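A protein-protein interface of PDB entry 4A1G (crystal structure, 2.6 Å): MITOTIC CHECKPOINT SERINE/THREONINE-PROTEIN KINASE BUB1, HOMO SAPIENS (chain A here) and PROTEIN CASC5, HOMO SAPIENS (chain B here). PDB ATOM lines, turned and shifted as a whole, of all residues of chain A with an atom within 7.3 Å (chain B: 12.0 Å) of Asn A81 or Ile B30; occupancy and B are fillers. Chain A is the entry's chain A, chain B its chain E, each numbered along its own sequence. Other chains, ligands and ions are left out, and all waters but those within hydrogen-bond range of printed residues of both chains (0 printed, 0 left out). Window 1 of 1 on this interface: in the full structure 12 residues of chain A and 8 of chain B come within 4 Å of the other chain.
The backbone carbonyl oxygen of Tyr A80 is in hydrogen-bond range of the backbone NH of Ile B30 (2.8 Å).
The side-chain amino group of Lys B29 lies within hydrogen-bond range of the backbone carbonyl oxygen of Glu A79 (2.7 Å).
The side-chain amide nitrogen (NE2) of Gln A86 lies within hydrogen-bond range of the side-chain hydroxyl (OG1) of Thr B33 (3.2 Å).
The side-chain amide nitrogen (NE2) of Gln A86 sits at hydrogen-bond distance from the side-chain hydroxyl (OG1) of Thr B32 (3.4 Å).
The backbone NH of Ser A82 lies within hydrogen-bond range of the backbone carbonyl oxygen of Ile B30, 3.0 Å away.
The backbone NH (N) of Thr B32 is in hydrogen-bond range of the side-chain hydroxyl (OG) of Ser A82 (3.1 Å).
N of Thr B33 sits close to OD1 of Asp B31, at 3.3 Å.
The side-chain hydroxyl (OG) of Ser B34 is in hydrogen-bond range of the side-chain carboxylate (OD1) of Asp B31.
The side-chain amide nitrogen of Asn A81 is in hydrogen-bond range of the backbone carbonyl oxygen of Phe A77, 2.8 Å away.
The side-chain amide nitrogen of Gln A86 is in hydrogen-bond range of the side-chain carboxylate of Asp A83 (2.9 Å).
Ile B30 touches Ile A48.
Phe B35 touches Glu A52.
Met A55 touches Phe B35 (CB to CZ, 3.98 Å).
Phe A77 touches Ile B30.
Phe B35 touches Phe A77.
Asn A81 touches Lys B29.
Ile B30 touches Asn A81 (CD1 to OD1, 3.5 Å).
OG of Ser A82 touches CA of Asp B31, 3.6 Å away.
CG2 of Thr B32 touches N of Asp A83, at 3.0 Å.
CD2 of Leu B36 touches OE1 of Gln A86, 3.6 Å away.
Ile A48 touches just one residue of chain B: Ile B30.
Lys A76 touches none of the printed residues of chain B.
No residue of chain B comes within 4 Å of Ala A78.
Of the printed residues of chain B, Asn A81 touches Lys B29 (3.5 Å), Ile B30 (3.5 Å) and Thr B32 (2.9 Å).
Ser A82 touches three residues of chain B.
Of the printed residues of chain B, Gln A86 touches Thr B32 (3.4 Å), Thr B33 (3.2 Å) and Leu B36 (3.6 Å).
No residue of chain B comes within 4 Å of Phe A87.
Of the printed residues of chain A, Lys B29 touches Glu A79, Tyr A80 and Asn A81.
Of the printed residues of chain A, Ile B30 touches Ile A48, Phe A77, Tyr A80, Asn A81 and Ser A82.
Of the printed residues of chain A, Thr B32 touches Asn A81, Ser A82, Asp A83 and Gln A86.
Printed residues of chain A within 4 Å of Phe B35: Glu A52 (3.8 Å), Met A55 (3.98 Å) and Phe A77 (3.6 Å).
Printed residues of chain A within 4 Å of Leu B36: Gln A86.
Ala B37 touches none of the printed residues of chain A.
The nearest printed residue of chain A that does not touch Ile B30 is Glu A52 (4.01 Å).
The nearest printed residue of chain B that does not touch Glu A79 is Ile B30 (6.9 Å).
Hydrophobic or aromatic side chains of chain A that line the printed part of chain B: Ile A48, Met A55 and Phe A77.
Printed residues of chain B that touch a printed residue of chain A: Lys B29, Ile B30, Asp B31, Thr B32, Thr B33, Phe B35 and Leu B36.
Among the printed residues, 18 pairs touch across the chains.
Among the printed residues, no Asp or Glu carboxylate lies within 4 Å of a Lys or Arg side-chain nitrogen of the other chain.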
ATOM      1  N   ILE A  48      14.584  -9.515 -20.163  1.00  0.00           N
ATOM      2  CA  ILE A  48      13.559 -10.544 -20.036  1.00  0.00           C
ATOM      3  C   ILE A  48      12.468 -10.416 -21.079  1.00  0.00           C
ATOM      4  O   ILE A  48      12.028 -11.411 -21.669  1.00  0.00           O
ATOM      5  CB  ILE A  48      12.889 -10.507 -18.674  1.00  0.00           C
ATOM      6  CG1 ILE A  48      13.887 -10.886 -17.588  1.00  0.00           C
ATOM      7  CG2 ILE A  48      11.706 -11.456 -18.640  1.00  0.00           C
ATOM      8  CD1 ILE A  48      13.226 -11.338 -16.323  1.00  0.00           C
ATOM      9  N   GLU A  52      11.912 -13.170 -23.967  1.00  0.00           N
ATOM     10  CA  GLU A  52      10.621 -13.837 -24.164  1.00  0.00           C
ATOM     11  C   GLU A  52      10.098 -13.722 -25.593  1.00  0.00           C
ATOM     12  O   GLU A  52       9.583 -14.696 -26.157  1.00  0.00           O
ATOM     13  CB  GLU A  52       9.583 -13.282 -23.215  1.00  0.00           C
ATOM     14  CG  GLU A  52       9.858 -13.558 -21.764  1.00  0.00           C
ATOM     15  CD  GLU A  52       8.656 -13.228 -20.923  1.00  0.00           C
ATOM     16  OE1 GLU A  52       7.755 -12.548 -21.465  1.00  0.00           O
ATOM     17  OE2 GLU A  52       8.602 -13.649 -19.746  1.00  0.00           O
ATOM     18  N   MET A  55      12.029 -15.899 -28.189  1.00  0.00           N
ATOM     19  CA  MET A  55      11.519 -17.266 -28.193  1.00  0.00           C
ATOM     20  C   MET A  55      10.281 -17.407 -29.025  1.00  0.00           C
ATOM     21  O   MET A  55      10.226 -18.222 -29.941  1.00  0.00           O
ATOM     22  CB  MET A  55      11.118 -17.660 -26.790  1.00  0.00           C
ATOM     23  CG  MET A  55      12.245 -17.622 -25.824  1.00  0.00           C
ATOM     24  SD  MET A  55      12.881 -19.245 -25.437  1.00  0.00           S
ATOM     25  CE  MET A  55      14.432 -18.693 -24.729  1.00  0.00           C
ATOM     26  N   CYS A  74      18.913 -18.627 -25.317  1.00  0.00           N
ATOM     27  CA  CYS A  74      18.084 -19.581 -24.611  1.00  0.00           C
ATOM     28  C   CYS A  74      18.670 -19.901 -23.244  1.00  0.00           C
ATOM     29  O   CYS A  74      17.947 -19.906 -22.244  1.00  0.00           O
ATOM     30  CB  CYS A  74      17.846 -20.837 -25.455  1.00  0.00           C
ATOM     31  SG  CYS A  74      16.578 -20.586 -26.708  1.00  0.00           S
ATOM     32  N   LEU A  75      19.979 -20.144 -23.200  1.00  0.00           N
ATOM     33  CA  LEU A  75      20.697 -20.355 -21.926  1.00  0.00           C
ATOM     34  C   LEU A  75      20.689 -19.120 -21.028  1.00  0.00           C
ATOM     35  O   LEU A  75      20.501 -19.216 -19.807  1.00  0.00           O
ATOM     36  CB  LEU A  75      22.148 -20.760 -22.193  1.00  0.00           C
ATOM     37  CG  LEU A  75      22.537 -22.237 -22.142  1.00  0.00           C
ATOM     38  CD1 LEU A  75      21.379 -23.116 -22.511  1.00  0.00           C
ATOM     39  CD2 LEU A  75      23.730 -22.503 -23.038  1.00  0.00           C
ATOM     40  N   LYS A  76      20.926 -17.960 -21.637  1.00  0.00           N
ATOM     41  CA  LYS A  76      20.786 -16.681 -20.946  1.00  0.00           C
ATOM     42  C   LYS A  76      19.424 -16.578 -20.262  1.00  0.00           C
ATOM     43  O   LYS A  76      19.343 -16.302 -19.074  1.00  0.00           O
ATOM     44  CB  LYS A  76      20.933 -15.545 -21.950  1.00  0.00           C
ATOM     45  CG  LYS A  76      21.951 -14.505 -21.573  1.00  0.00           C
ATOM     46  CD  LYS A  76      22.977 -14.374 -22.699  1.00  0.00           C
ATOM     47  CE  LYS A  76      23.717 -13.059 -22.651  1.00  0.00           C
ATOM     48  NZ  LYS A  76      24.125 -12.679 -24.024  1.00  0.00           N
ATOM     49  N   PHE A  77      18.358 -16.809 -21.023  1.00  0.00           N
ATOM     50  CA  PHE A  77      16.989 -16.673 -20.528  1.00  0.00           C
ATOM     51  C   PHE A  77      16.645 -17.687 -19.453  1.00  0.00           C
ATOM     52  O   PHE A  77      15.786 -17.443 -18.608  1.00  0.00           O
ATOM     53  CB  PHE A  77      16.018 -16.824 -21.694  1.00  0.00           C
ATOM     54  CG  PHE A  77      14.568 -16.741 -21.310  1.00  0.00           C
ATOM     55  CD1 PHE A  77      14.069 -15.636 -20.644  1.00  0.00           C
ATOM     56  CD2 PHE A  77      13.683 -17.749 -21.672  1.00  0.00           C
ATOM     57  CE1 PHE A  77      12.718 -15.551 -20.318  1.00  0.00           C
ATOM     58  CE2 PHE A  77      12.327 -17.664 -21.348  1.00  0.00           C
ATOM     59  CZ  PHE A  77      11.851 -16.567 -20.673  1.00  0.00           C
ATOM     60  N   ALA A  78      17.298 -18.839 -19.505  1.00  0.00           N
ATOM     61  CA  ALA A  78      17.075 -19.867 -18.503  1.00  0.00           C
ATOM     62  C   ALA A  78      17.288 -19.274 -17.109  1.00  0.00           C
ATOM     63  O   ALA A  78      16.557 -19.583 -16.172  1.00  0.00           O
ATOM     64  CB  ALA A  78      18.003 -21.014 -18.732  1.00  0.00           C
ATOM     65  N   GLU A  79      18.291 -18.409 -16.983  1.00  0.00           N
ATOM     66  CA  GLU A  79      18.612 -17.770 -15.709  1.00  0.00           C
ATOM     67  C   GLU A  79      17.413 -17.039 -15.076  1.00  0.00           C
ATOM     68  O   GLU A  79      17.319 -16.906 -13.854  1.00  0.00           O
ATOM     69  CB  GLU A  79      19.781 -16.812 -15.888  1.00  0.00           C
ATOM     70  CG  GLU A  79      19.907 -15.777 -14.791  1.00  0.00           C
ATOM     71  CD  GLU A  79      21.050 -14.808 -15.049  1.00  0.00           C
ATOM     72  OE1 GLU A  79      21.833 -15.062 -16.007  1.00  0.00           O
ATOM     73  OE2 GLU A  79      21.161 -13.801 -14.301  1.00  0.00           O
ATOM     74  N   TYR A  80      16.479 -16.588 -15.900  1.00  0.00           N
ATOM     75  CA  TYR A  80      15.329 -15.871 -15.371  1.00  0.00           C
ATOM     76  C   TYR A  80      14.103 -16.767 -15.207  1.00  0.00           C
ATOM     77  O   TYR A  80      13.037 -16.298 -14.844  1.00  0.00           O
ATOM     78  CB  TYR A  80      15.030 -14.663 -16.248  1.00  0.00           C
ATOM     79  CG  TYR A  80      16.264 -13.837 -16.478  1.00  0.00           C
ATOM     80  CD1 TYR A  80      16.796 -13.058 -15.464  1.00  0.00           C
ATOM     81  CD2 TYR A  80      16.923 -13.862 -17.696  1.00  0.00           C
ATOM     82  CE1 TYR A  80      17.930 -12.310 -15.655  1.00  0.00           C
ATOM     83  CE2 TYR A  80      18.069 -13.116 -17.897  1.00  0.00           C
ATOM     84  CZ  TYR A  80      18.567 -12.340 -16.869  1.00  0.00           C
ATOM     85  OH  TYR A  80      19.707 -11.587 -17.056  1.00  0.00           O
ATOM     86  N   ASN A  81      14.263 -18.060 -15.457  1.00  0.00           N
ATOM     87  CA  ASN A  81      13.142 -18.994 -15.373  1.00  0.00           C
ATOM     88  C   ASN A  81      12.974 -19.549 -13.970  1.00  0.00           C
ATOM     89  O   ASN A  81      13.954 -19.775 -13.275  1.00  0.00           O
ATOM     90  CB  ASN A  81      13.310 -20.140 -16.383  1.00  0.00           C
ATOM     91  CG  ASN A  81      12.742 -19.803 -17.749  1.00  0.00           C
ATOM     92  OD1 ASN A  81      11.626 -20.202 -18.077  1.00  0.00           O
ATOM     93  ND2 ASN A  81      13.497 -19.056 -18.546  1.00  0.00           N
ATOM     94  N   SER A  82      11.733 -19.771 -13.552  1.00  0.00           N
ATOM     95  CA  SER A  82      11.471 -20.347 -12.233  1.00  0.00           C
ATOM     96  C   SER A  82      11.749 -21.849 -12.167  1.00  0.00           C
ATOM     97  O   SER A  82      12.173 -22.354 -11.133  1.00  0.00           O
ATOM     98  CB  SER A  82      10.022 -20.100 -11.827  1.00  0.00           C
ATOM     99  OG  SER A  82       9.119 -20.711 -12.737  1.00  0.00           O
ATOM    100  N   ASP A  83      11.506 -22.559 -13.268  1.00  0.00           N
ATOM    101  CA  ASP A  83      11.531 -24.023 -13.278  1.00  0.00           C
ATOM    102  C   ASP A  83      12.453 -24.584 -14.355  1.00  0.00           C
ATOM    103  O   ASP A  83      12.021 -24.883 -15.463  1.00  0.00           O
ATOM    104  CB  ASP A  83      10.117 -24.555 -13.489  1.00  0.00           C
ATOM    105  CG  ASP A  83      10.060 -26.064 -13.553  1.00  0.00           C
ATOM    106  OD1 ASP A  83      11.132 -26.702 -13.585  1.00  0.00           O
ATOM    107  OD2 ASP A  83       8.934 -26.619 -13.581  1.00  0.00           O
ATOM    108  N   LEU A  84      13.720 -24.746 -14.014  1.00  0.00           N
ATOM    109  CA  LEU A  84      14.723 -25.153 -14.985  1.00  0.00           C
ATOM    110  C   LEU A  84      14.483 -26.544 -15.593  1.00  0.00           C
ATOM    111  O   LEU A  84      14.837 -26.784 -16.751  1.00  0.00           O
ATOM    112  CB  LEU A  84      16.121 -25.053 -14.363  1.00  0.00           C
ATOM    113  CG  LEU A  84      16.970 -23.845 -14.755  1.00  0.00           C
ATOM    114  CD1 LEU A  84      16.115 -22.669 -15.139  1.00  0.00           C
ATOM    115  CD2 LEU A  84      17.896 -23.481 -13.624  1.00  0.00           C
ATOM    116  N   GLN A  86      11.544 -27.936 -16.260  1.00  0.00           N
ATOM    117  CA  GLN A  86      10.538 -27.763 -17.278  1.00  0.00           C
ATOM    118  C   GLN A  86      11.136 -27.035 -18.467  1.00  0.00           C
ATOM    119  O   GLN A  86      10.920 -27.420 -19.613  1.00  0.00           O
ATOM    120  CB  GLN A  86       9.356 -26.987 -16.710  1.00  0.00           C
ATOM    121  CG  GLN A  86       8.179 -26.908 -17.645  1.00  0.00           C
ATOM    122  CD  GLN A  86       7.034 -26.143 -17.047  1.00  0.00           C
ATOM    123  OE1 GLN A  86       6.093 -25.767 -17.749  1.00  0.00           O
ATOM    124  NE2 GLN A  86       7.102 -25.902 -15.735  1.00  0.00           N
ATOM    125  N   PHE A  87      11.902 -25.986 -18.195  1.00  0.00           N
ATOM    126  CA  PHE A  87      12.427 -25.160 -19.269  1.00  0.00           C
ATOM    127  C   PHE A  87      13.315 -25.969 -20.195  1.00  0.00           C
ATOM    128  O   PHE A  87      13.076 -25.998 -21.393  1.00  0.00           O
ATOM    129  CB  PHE A  87      13.171 -23.935 -18.735  1.00  0.00           C
ATOM    130  CG  PHE A  87      13.588 -22.975 -19.811  1.00  0.00           C
ATOM    131  CD1 PHE A  87      12.644 -22.302 -20.560  1.00  0.00           C
ATOM    132  CD2 PHE A  87      14.924 -22.758 -20.092  1.00  0.00           C
ATOM    133  CE1 PHE A  87      13.025 -21.433 -21.555  1.00  0.00           C
ATOM    134  CE2 PHE A  87      15.307 -21.887 -21.091  1.00  0.00           C
ATOM    135  CZ  PHE A  87      14.359 -21.230 -21.821  1.00  0.00           C
ATOM    136  N   PHE A  88      14.332 -26.627 -19.643  1.00  0.00           N
ATOM    137  CA  PHE A  88      15.263 -27.400 -20.460  1.00  0.00           C
ATOM    138  C   PHE A  88      14.549 -28.479 -21.256  1.00  0.00           C
ATOM    139  O   PHE A  88      14.884 -28.733 -22.424  1.00  0.00           O
ATOM    140  CB  PHE A  88      16.356 -28.053 -19.611  1.00  0.00           C
ATOM    141  CG  PHE A  88      17.438 -27.114 -19.201  1.00  0.00           C
ATOM    142  CD1 PHE A  88      18.175 -26.426 -20.164  1.00  0.00           C
ATOM    143  CD2 PHE A  88      17.723 -26.912 -17.846  1.00  0.00           C
ATOM    144  CE1 PHE A  88      19.183 -25.545 -19.780  1.00  0.00           C
ATOM    145  CE2 PHE A  88      18.722 -26.028 -17.450  1.00  0.00           C
ATOM    146  CZ  PHE A  88      19.460 -25.345 -18.411  1.00  0.00           C
ATOM    147  N   LYS B  29      12.772 -13.309 -11.586  1.00  0.00           N
ATOM    148  CA  LYS B  29      12.332 -14.550 -12.221  1.00  0.00           C
ATOM    149  C   LYS B  29      10.914 -14.500 -12.795  1.00  0.00           C
ATOM    150  O   LYS B  29      10.092 -13.692 -12.375  1.00  0.00           O
ATOM    151  CB  LYS B  29      12.466 -15.715 -11.247  1.00  0.00           C
ATOM    152  CG  LYS B  29      13.907 -16.032 -10.941  1.00  0.00           C
ATOM    153  CD  LYS B  29      14.044 -17.240 -10.057  1.00  0.00           C
ATOM    154  CE  LYS B  29      15.204 -18.073 -10.533  1.00  0.00           C
ATOM    155  NZ  LYS B  29      16.059 -17.279 -11.455  1.00  0.00           N
ATOM    156  N   ILE B  30      10.643 -15.366 -13.768  1.00  0.00           N
ATOM    157  CA  ILE B  30       9.323 -15.456 -14.374  1.00  0.00           C
ATOM    158  C   ILE B  30       8.785 -16.866 -14.196  1.00  0.00           C
ATOM    159  O   ILE B  30       9.541 -17.799 -13.926  1.00  0.00           O
ATOM    160  CB  ILE B  30       9.332 -15.089 -15.888  1.00  0.00           C
ATOM    161  CG1 ILE B  30       9.054 -16.313 -16.780  1.00  0.00           C
ATOM    162  CG2 ILE B  30      10.608 -14.355 -16.270  1.00  0.00           C
ATOM    163  CD1 ILE B  30      10.248 -17.179 -17.062  1.00  0.00           C
ATOM    164  N   ASP B  31       7.477 -17.024 -14.341  1.00  0.00           N
ATOM    165  CA  ASP B  31       6.889 -18.337 -14.170  1.00  0.00           C
ATOM    166  C   ASP B  31       6.975 -19.109 -15.471  1.00  0.00           C
ATOM    167  O   ASP B  31       6.270 -18.793 -16.435  1.00  0.00           O
ATOM    168  CB  ASP B  31       5.436 -18.238 -13.711  1.00  0.00           C
ATOM    169  CG  ASP B  31       4.890 -19.576 -13.248  1.00  0.00           C
ATOM    170  OD1 ASP B  31       4.374 -20.345 -14.093  1.00  0.00           O
ATOM    171  OD2 ASP B  31       4.991 -19.861 -12.034  1.00  0.00           O
ATOM    172  N   THR B  32       7.829 -20.130 -15.491  1.00  0.00           N
ATOM    173  CA  THR B  32       8.080 -20.849 -16.729  1.00  0.00           C
ATOM    174  C   THR B  32       6.828 -21.574 -17.208  1.00  0.00           C
ATOM    175  O   THR B  32       6.568 -21.628 -18.408  1.00  0.00           O
ATOM    176  CB  THR B  32       9.342 -21.785 -16.674  1.00  0.00           C
ATOM    177  OG1 THR B  32       8.976 -23.116 -16.307  1.00  0.00           O
ATOM    178  CG2 THR B  32      10.358 -21.264 -15.701  1.00  0.00           C
ATOM    179  N   THR B  33       6.027 -22.091 -16.283  1.00  0.00           N
ATOM    180  CA  THR B  33       4.802 -22.796 -16.681  1.00  0.00           C
ATOM    181  C   THR B  33       3.861 -21.898 -17.484  1.00  0.00           C
ATOM    182  O   THR B  33       3.446 -22.254 -18.592  1.00  0.00           O
ATOM    183  CB  THR B  33       4.035 -23.371 -15.483  1.00  0.00           C
ATOM    184  OG1 THR B  33       4.957 -23.868 -14.502  1.00  0.00           O
ATOM    185  CG2 THR B  33       3.135 -24.490 -15.953  1.00  0.00           C
ATOM    186  N   SER B  34       3.539 -20.736 -16.916  1.00  0.00           N
ATOM    187  CA  SER B  34       2.726 -19.723 -17.596  1.00  0.00           C
ATOM    188  C   SER B  34       3.356 -19.316 -18.916  1.00  0.00           C
ATOM    189  O   SER B  34       2.673 -19.223 -19.940  1.00  0.00           O
ATOM    190  CB  SER B  34       2.569 -18.481 -16.725  1.00  0.00           C
ATOM    191  OG  SER B  34       2.435 -18.837 -15.360  1.00  0.00           O
ATOM    192  N   PHE B  35       4.663 -19.074 -18.885  1.00  0.00           N
ATOM    193  CA  PHE B  35       5.368 -18.645 -20.079  1.00  0.00           C
ATOM    194  C   PHE B  35       5.275 -19.657 -21.222  1.00  0.00           C
ATOM    195  O   PHE B  35       4.995 -19.296 -22.364  1.00  0.00           O
ATOM    196  CB  PHE B  35       6.835 -18.348 -19.789  1.00  0.00           C
ATOM    197  CG  PHE B  35       7.629 -18.127 -21.030  1.00  0.00           C
ATOM    198  CD1 PHE B  35       7.420 -16.989 -21.800  1.00  0.00           C
ATOM    199  CD2 PHE B  35       8.528 -19.082 -21.473  1.00  0.00           C
ATOM    200  CE1 PHE B  35       8.122 -16.783 -22.975  1.00  0.00           C
ATOM    201  CE2 PHE B  35       9.231 -18.890 -22.648  1.00  0.00           C
ATOM    202  CZ  PHE B  35       9.031 -17.733 -23.403  1.00  0.00           C
ATOM    203  N   LEU B  36       5.537 -20.919 -20.906  1.00  0.00           N
ATOM    204  CA  LEU B  36       5.537 -21.975 -21.910  1.00  0.00           C
ATOM    205  C   LEU B  36       4.134 -22.230 -22.415  1.00  0.00           C
ATOM    206  O   LEU B  36       3.938 -22.509 -23.599  1.00  0.00           O
ATOM    207  CB  LEU B  36       6.090 -23.266 -21.321  1.00  0.00           C
ATOM    208  CG  LEU B  36       7.594 -23.480 -21.371  1.00  0.00           C
ATOM    209  CD1 LEU B  36       8.285 -22.282 -21.969  1.00  0.00           C
ATOM    210  CD2 LEU B  36       8.080 -23.778 -19.958  1.00  0.00           C
ATOM    211  N   ALA B  37       3.165 -22.150 -21.504  1.00  0.00           N
ATOM    212  CA  ALA B  37       1.756 -22.297 -21.861  1.00  0.00           C
ATOM    213  C   ALA B  37       1.369 -21.331 -22.989  1.00  0.00           C
ATOM    214  O   ALA B  37       0.901 -21.759 -24.049  1.00  0.00           O
ATOM    215  CB  ALA B  37       0.872 -22.094 -20.637  1.00  0.00           C
ATOM    216  N   ASN B  38       1.574 -20.035 -22.763  1.00  0.00           N
ATOM    217  CA  ASN B  38       1.391 -19.033 -23.810  1.00  0.00           C
ATOM    218  C   ASN B  38       2.003 -19.487 -25.151  1.00  0.00           C
ATOM    219  O   ASN B  38       1.572 -19.053 -26.221  1.00  0.00           O
ATOM    220  CB  ASN B  38       1.970 -17.685 -23.353  1.00  0.00           C
ATOM    221  CG  ASN B  38       1.684 -16.543 -24.332  1.00  0.00           C
ATOM    222  OD1 ASN B  38       1.024 -15.561 -23.976  1.00  0.00           O
ATOM    223  ND2 ASN B  38       2.193 -16.657 -25.561  1.00  0.00           N
ATOM    224  N   LEU B  39       2.995 -20.374 -25.089  1.00  0.00           N
ATOM    225  CA  LEU B  39       3.615 -20.919 -26.296  1.00  0.00           C
ATOM    226  C   LEU B  39       2.975 -22.245 -26.755  1.00  0.00           C
ATOM    227  O   LEU B  39       3.406 -23.335 -26.357  1.00  0.00           O
ATOM    228  CB  LEU B  39       5.128 -21.080 -26.093  1.00  0.00           C
ATOM    229  CG  LEU B  39       5.869 -19.770 -25.824  1.00  0.00           C
ATOM    230  CD1 LEU B  39       7.354 -19.928 -26.034  1.00  0.00           C
ATOM    231  CD2 LEU B  39       5.320 -18.707 -26.742  1.00  0.00           C
